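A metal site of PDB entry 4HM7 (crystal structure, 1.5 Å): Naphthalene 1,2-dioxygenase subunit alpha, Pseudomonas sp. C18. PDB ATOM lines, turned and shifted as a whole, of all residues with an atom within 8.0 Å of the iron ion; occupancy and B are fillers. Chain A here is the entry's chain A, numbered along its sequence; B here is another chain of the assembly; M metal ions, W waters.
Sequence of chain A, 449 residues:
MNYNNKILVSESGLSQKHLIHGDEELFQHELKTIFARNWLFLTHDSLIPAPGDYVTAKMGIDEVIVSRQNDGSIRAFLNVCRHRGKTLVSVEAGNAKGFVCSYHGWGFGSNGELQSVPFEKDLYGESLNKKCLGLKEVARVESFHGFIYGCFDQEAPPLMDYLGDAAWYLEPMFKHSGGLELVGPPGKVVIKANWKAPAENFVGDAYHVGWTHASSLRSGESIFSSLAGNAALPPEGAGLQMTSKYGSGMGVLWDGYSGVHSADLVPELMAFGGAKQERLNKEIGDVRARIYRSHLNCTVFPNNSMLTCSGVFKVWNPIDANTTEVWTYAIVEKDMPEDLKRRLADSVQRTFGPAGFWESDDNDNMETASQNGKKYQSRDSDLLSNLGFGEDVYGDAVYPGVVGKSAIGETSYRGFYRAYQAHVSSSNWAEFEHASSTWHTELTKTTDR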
ATOM      1  N   ASN A 201       6.013  19.238   7.578  1.00  0.00           N
ATOM      2  CA  ASN A 201       6.973  18.192   7.327  1.00  0.00           C
ATOM      3  C   ASN A 201       7.482  18.268   5.885  1.00  0.00           C
ATOM      4  O   ASN A 201       8.687  18.221   5.642  1.00  0.00           O
ATOM      5  CB  ASN A 201       6.337  16.834   7.621  1.00  0.00           C
ATOM      6  CG  ASN A 201       7.261  15.686   7.358  1.00  0.00           C
ATOM      7  OD1 ASN A 201       8.018  15.274   8.233  1.00  0.00           O
ATOM      8  ND2 ASN A 201       7.197  15.144   6.151  1.00  0.00           N
ATOM      9  N   PHE A 202       6.565  18.413   4.940  1.00  0.00           N
ATOM     10  CA  PHE A 202       6.973  18.544   3.544  1.00  0.00           C
ATOM     11  C   PHE A 202       7.659  19.864   3.213  1.00  0.00           C
ATOM     12  O   PHE A 202       8.502  19.912   2.314  1.00  0.00           O
ATOM     13  CB  PHE A 202       5.792  18.332   2.597  1.00  0.00           C
ATOM     14  CG  PHE A 202       5.497  16.887   2.313  1.00  0.00           C
ATOM     15  CD1 PHE A 202       5.128  16.026   3.342  1.00  0.00           C
ATOM     16  CD2 PHE A 202       5.598  16.379   1.024  1.00  0.00           C
ATOM     17  CE1 PHE A 202       4.849  14.689   3.084  1.00  0.00           C
ATOM     18  CE2 PHE A 202       5.318  15.045   0.756  1.00  0.00           C
ATOM     19  CZ  PHE A 202       4.949  14.190   1.798  1.00  0.00           C
ATOM     20  N   ASP A 205      11.272  19.718   6.364  1.00  0.00           N
ATOM     21  CA  ASP A 205      11.806  18.717   7.273  1.00  0.00           C
ATOM     22  C   ASP A 205      12.669  17.666   6.593  1.00  0.00           C
ATOM     23  O   ASP A 205      12.206  16.555   6.273  1.00  0.00           O
ATOM     24  CB  ASP A 205      10.666  18.060   8.035  1.00  0.00           C
ATOM     25  CG  ASP A 205      11.123  17.252   9.237  1.00  0.00           C
ATOM     26  OD1 ASP A 205      12.325  16.911   9.328  1.00  0.00           O
ATOM     27  OD2 ASP A 205      10.260  16.952  10.093  1.00  0.00           O
ATOM     28  N   HIS A 208      14.159  14.762   9.604  1.00  0.00           N
ATOM     29  CA  HIS A 208      13.472  13.539  10.021  1.00  0.00           C
ATOM     30  C   HIS A 208      13.801  12.343   9.130  1.00  0.00           C
ATOM     31  O   HIS A 208      13.610  11.204   9.536  1.00  0.00           O
ATOM     32  CB  HIS A 208      11.952  13.735  10.078  1.00  0.00           C
ATOM     33  CG  HIS A 208      11.238  13.503   8.770  1.00  0.00           C
ATOM     34  ND1 HIS A 208      11.344  14.371   7.695  1.00  0.00           N
ATOM     35  CD2 HIS A 208      10.396  12.520   8.378  1.00  0.00           C
ATOM     36  CE1 HIS A 208      10.613  13.908   6.691  1.00  0.00           C
ATOM     37  NE2 HIS A 208      10.030  12.792   7.085  1.00  0.00           N
ATOM     38  N   VAL A 209      14.291  12.593   7.918  1.00  0.00           N
ATOM     39  CA  VAL A 209      14.339  11.536   6.900  1.00  0.00           C
ATOM     40  C   VAL A 209      15.154  10.301   7.312  1.00  0.00           C
ATOM     41  O   VAL A 209      14.652   9.183   7.225  1.00  0.00           O
ATOM     42  CB  VAL A 209      14.779  12.070   5.534  1.00  0.00           C
ATOM     43  CG1 VAL A 209      14.922  10.916   4.531  1.00  0.00           C
ATOM     44  CG2 VAL A 209      13.779  13.107   5.033  1.00  0.00           C
ATOM     45  N   THR A 212      13.175   8.793  10.857  1.00  0.00           N
ATOM     46  CA  THR A 212      11.793   8.358  10.608  1.00  0.00           C
ATOM     47  C   THR A 212      11.739   7.274   9.534  1.00  0.00           C
ATOM     48  O   THR A 212      11.072   6.251   9.711  1.00  0.00           O
ATOM     49  CB  THR A 212      10.908   9.539  10.160  1.00  0.00           C
ATOM     50  OG1 THR A 212      10.672  10.409  11.273  1.00  0.00           O
ATOM     51  CG2 THR A 212       9.547   9.037   9.644  1.00  0.00           C
ATOM     52  N   HIS A 213      12.456   7.490   8.445  1.00  0.00           N
ATOM     53  CA  HIS A 213      12.359   6.614   7.286  1.00  0.00           C
ATOM     54  C   HIS A 213      13.494   5.610   7.208  1.00  0.00           C
ATOM     55  O   HIS A 213      13.757   5.054   6.137  1.00  0.00           O
ATOM     56  CB  HIS A 213      12.267   7.436   5.984  1.00  0.00           C
ATOM     57  CG  HIS A 213      11.043   8.289   5.910  1.00  0.00           C
ATOM     58  ND1 HIS A 213       9.770   7.766   5.804  1.00  0.00           N
ATOM     59  CD2 HIS A 213      10.890   9.634   5.920  1.00  0.00           C
ATOM     60  CE1 HIS A 213       8.891   8.745   5.763  1.00  0.00           C
ATOM     61  NE2 HIS A 213       9.542   9.895   5.832  1.00  0.00           N
ATOM     62  N   LEU A 307       6.829  16.326  -3.717  1.00  0.00           N
ATOM     63  CA  LEU A 307       8.242  15.984  -3.850  1.00  0.00           C
ATOM     64  C   LEU A 307       8.475  15.917  -5.335  1.00  0.00           C
ATOM     65  O   LEU A 307       7.989  14.998  -6.001  1.00  0.00           O
ATOM     66  CB  LEU A 307       8.522  14.599  -3.237  1.00  0.00           C
ATOM     67  CG  LEU A 307       8.080  14.403  -1.776  1.00  0.00           C
ATOM     68  CD1 LEU A 307       8.357  12.994  -1.245  1.00  0.00           C
ATOM     69  CD2 LEU A 307       8.720  15.451  -0.854  1.00  0.00           C
ATOM     70  N   PHE A 352       4.330   6.495  -1.268  1.00  0.00           N
ATOM     71  CA  PHE A 352       3.638   7.569  -0.547  1.00  0.00           C
ATOM     72  C   PHE A 352       2.111   7.550  -0.668  1.00  0.00           C
ATOM     73  O   PHE A 352       1.446   8.478  -0.198  1.00  0.00           O
ATOM     74  CB  PHE A 352       4.189   8.937  -0.970  1.00  0.00           C
ATOM     75  CG  PHE A 352       5.443   9.322  -0.244  1.00  0.00           C
ATOM     76  CD1 PHE A 352       6.685   8.908  -0.709  1.00  0.00           C
ATOM     77  CD2 PHE A 352       5.385  10.076   0.915  1.00  0.00           C
ATOM     78  CE1 PHE A 352       7.849   9.254  -0.033  1.00  0.00           C
ATOM     79  CE2 PHE A 352       6.539  10.428   1.603  1.00  0.00           C
ATOM     80  CZ  PHE A 352       7.771  10.017   1.129  1.00  0.00           C
ATOM     81  N   TRP A 358       6.768   4.402   2.800  1.00  0.00           N
ATOM     82  CA  TRP A 358       7.415   5.612   3.344  1.00  0.00           C
ATOM     83  C   TRP A 358       6.408   6.436   4.146  1.00  0.00           C
ATOM     84  O   TRP A 358       6.677   6.817   5.286  1.00  0.00           O
ATOM     85  CB  TRP A 358       8.000   6.486   2.233  1.00  0.00           C
ATOM     86  CG  TRP A 358       9.218   5.962   1.531  1.00  0.00           C
ATOM     87  CD1 TRP A 358       9.297   4.854   0.727  1.00  0.00           C
ATOM     88  CD2 TRP A 358      10.512   6.560   1.513  1.00  0.00           C
ATOM     89  NE1 TRP A 358      10.575   4.718   0.227  1.00  0.00           N
ATOM     90  CE2 TRP A 358      11.338   5.756   0.695  1.00  0.00           C
ATOM     91  CE3 TRP A 358      11.065   7.695   2.110  1.00  0.00           C
ATOM     92  CZ2 TRP A 358      12.688   6.045   0.474  1.00  0.00           C
ATOM     93  CZ3 TRP A 358      12.404   7.996   1.883  1.00  0.00           C
ATOM     94  CH2 TRP A 358      13.191   7.168   1.070  1.00  0.00           C
ATOM     95  N   GLU A 359       5.257   6.733   3.540  1.00  0.00           N
ATOM     96  CA  GLU A 359       4.263   7.571   4.210  1.00  0.00           C
ATOM     97  C   GLU A 359       3.815   6.955   5.538  1.00  0.00           C
ATOM     98  O   GLU A 359       3.531   7.675   6.497  1.00  0.00           O
ATOM     99  CB  GLU A 359       3.052   7.814   3.292  1.00  0.00           C
ATOM    100  CG  GLU A 359       1.909   8.608   3.923  1.00  0.00           C
ATOM    101  CD  GLU A 359       1.731   9.994   3.347  1.00  0.00           C
ATOM    102  OE1 GLU A 359       2.727  10.610   2.907  1.00  0.00           O
ATOM    103  OE2 GLU A 359       0.585  10.482   3.324  1.00  0.00           O
ATOM    104  N   SER A 360       3.779   5.633   5.598  1.00  0.00           N
ATOM    105  CA  SER A 360       3.390   4.956   6.829  1.00  0.00           C
ATOM    106  C   SER A 360       4.355   5.252   7.975  1.00  0.00           C
ATOM    107  O   SER A 360       3.939   5.315   9.141  1.00  0.00           O
ATOM    108  CB  SER A 360       3.252   3.445   6.630  1.00  0.00           C
ATOM    109  OG  SER A 360       4.511   2.804   6.552  1.00  0.00           O
ATOM    110  N   ASP A 361       5.635   5.446   7.651  1.00  0.00           N
ATOM    111  CA  ASP A 361       6.633   5.785   8.672  1.00  0.00           C
ATOM    112  C   ASP A 361       6.282   7.074   9.384  1.00  0.00           C
ATOM    113  O   ASP A 361       6.669   7.286  10.534  1.00  0.00           O
ATOM    114  CB  ASP A 361       8.031   5.987   8.059  1.00  0.00           C
ATOM    115  CG  ASP A 361       8.581   4.755   7.355  1.00  0.00           C
ATOM    116  OD1 ASP A 361       8.196   3.614   7.687  1.00  0.00           O
ATOM    117  OD2 ASP A 361       9.437   4.950   6.463  1.00  0.00           O
ATOM    118  N   ASP A 362       5.561   7.961   8.700  1.00  0.00           N
ATOM    119  CA  ASP A 362       5.241   9.281   9.230  1.00  0.00           C
ATOM    120  C   ASP A 362       3.991   9.331  10.080  1.00  0.00           C
ATOM    121  O   ASP A 362       3.806  10.292  10.808  1.00  0.00           O
ATOM    122  CB  ASP A 362       5.057  10.298   8.095  1.00  0.00           C
ATOM    123  CG  ASP A 362       6.335  10.634   7.386  1.00  0.00           C
ATOM    124  OD1 ASP A 362       7.236  11.219   8.020  1.00  0.00           O
ATOM    125  OD2 ASP A 362       6.429  10.344   6.171  1.00  0.00           O
ATOM    126  N   ASN A 363       3.132   8.317   9.964  1.00  0.00           N
ATOM    127  CA  ASN A 363       1.805   8.318  10.610  1.00  0.00           C
ATOM    128  C   ASN A 363       1.849   8.673  12.082  1.00  0.00           C
ATOM    129  O   ASN A 363       1.190   9.630  12.498  1.00  0.00           O
ATOM    130  CB  ASN A 363       1.134   6.942  10.519  1.00  0.00           C
ATOM    131  CG  ASN A 363       0.470   6.681   9.178  1.00  0.00           C
ATOM    132  OD1 ASN A 363      -0.160   5.634   8.995  1.00  0.00           O
ATOM    133  ND2 ASN A 363       0.599   7.618   8.241  1.00  0.00           N
ATOM    134  N   ASN A 365       4.205   9.887  13.980  1.00  0.00           N
ATOM    135  CA  ASN A 365       4.784  11.198  14.191  1.00  0.00           C
ATOM    136  C   ASN A 365       3.734  12.297  14.032  1.00  0.00           C
ATOM    137  O   ASN A 365       3.562  13.127  14.927  1.00  0.00           O
ATOM    138  CB  ASN A 365       5.965  11.456  13.239  1.00  0.00           C
ATOM    139  CG  ASN A 365       7.151  10.521  13.489  1.00  0.00           C
ATOM    140  OD1 ASN A 365       7.359  10.031  14.601  1.00  0.00           O
ATOM    141  ND2 ASN A 365       7.931  10.280  12.442  1.00  0.00           N
ATOM    142  N   MET A 366       3.027  12.301  12.900  1.00  0.00           N
ATOM    143  CA  MET A 366       2.026  13.362  12.671  1.00  0.00           C
ATOM    144  C   MET A 366       0.825  13.277  13.578  1.00  0.00           C
ATOM    145  O   MET A 366       0.326  14.295  14.048  1.00  0.00           O
ATOM    146  CB  MET A 366       1.486  13.376  11.247  1.00  0.00           C
ATOM    147  CG  MET A 366       2.271  12.644  10.246  1.00  0.00           C
ATOM    148  SD  MET A 366       2.667  13.733   8.922  1.00  0.00           S
ATOM    149  CE  MET A 366       3.574  14.910   9.895  1.00  0.00           C
ATOM    150  N   TYR B 103      10.829  10.649  15.629  1.00  0.00           N
ATOM    151  CA  TYR B 103      10.620  11.654  14.587  1.00  0.00           C
ATOM    152  C   TYR B 103      11.990  12.142  14.093  1.00  0.00           C
ATOM    153  O   TYR B 103      12.379  11.820  12.968  1.00  0.00           O
ATOM    154  CB  TYR B 103       9.717  12.774  15.092  1.00  0.00           C
ATOM    155  CG  TYR B 103       9.033  13.614  14.021  1.00  0.00           C
ATOM    156  CD1 TYR B 103       9.442  13.564  12.690  1.00  0.00           C
ATOM    157  CD2 TYR B 103       7.975  14.462  14.348  1.00  0.00           C
ATOM    158  CE1 TYR B 103       8.825  14.341  11.720  1.00  0.00           C
ATOM    159  CE2 TYR B 103       7.348  15.248  13.381  1.00  0.00           C
ATOM    160  CZ  TYR B 103       7.788  15.183  12.065  1.00  0.00           C
ATOM    161  OH  TYR B 103       7.162  15.953  11.114  1.00  0.00           O
HETATM  162 FE    FE M   1       8.526  11.596   6.203  1.00  0.00          FE
HETATM  163  O   HOH W   1       7.639  12.911   4.870  1.00  0.00           O
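ND1 of His 213 sits close to O of Trp 358 (3.3 Å).
A ring nitrogen (ND1) of His 213 sits at hydrogen-bond distance from the side-chain carboxylate (OD2) of Asp 361 (2.9 Å).
OD1 of Asn 201 sits close to ND1 of His 208.
The backbone carbonyl oxygen (O) of Asp 205 lies within hydrogen-bond range of a ring nitrogen (ND1) of His 208 (2.7 Å).
The side-chain amide oxygen (OD1) of Asn 201 is in hydrogen-bond range of the side-chain hydroxyl (OH) of Tyr 103 of chain B (3.1 Å).
OD1 of Asn 201 sits close to OD2 of Asp 205 (3.4 Å).
Asn 201 touches the iron ion (ND2 to FE, 3.8 Å).
Four residues have an atom within 4 Å of the iron ion: Asn 201, His 208, His 213 and Asp 362.
NE2 of His 213 binds the iron ion (2.0 Å).
The iron ion is bound by water W1.
The iron ion is bound by NE2 of His 208 (2.1 Å).
OD1 of Asp 362 is bound to the iron ion, at 2.3 Å.
The iron ion is bound by OD2 of Asp 362 (2.4 Å).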
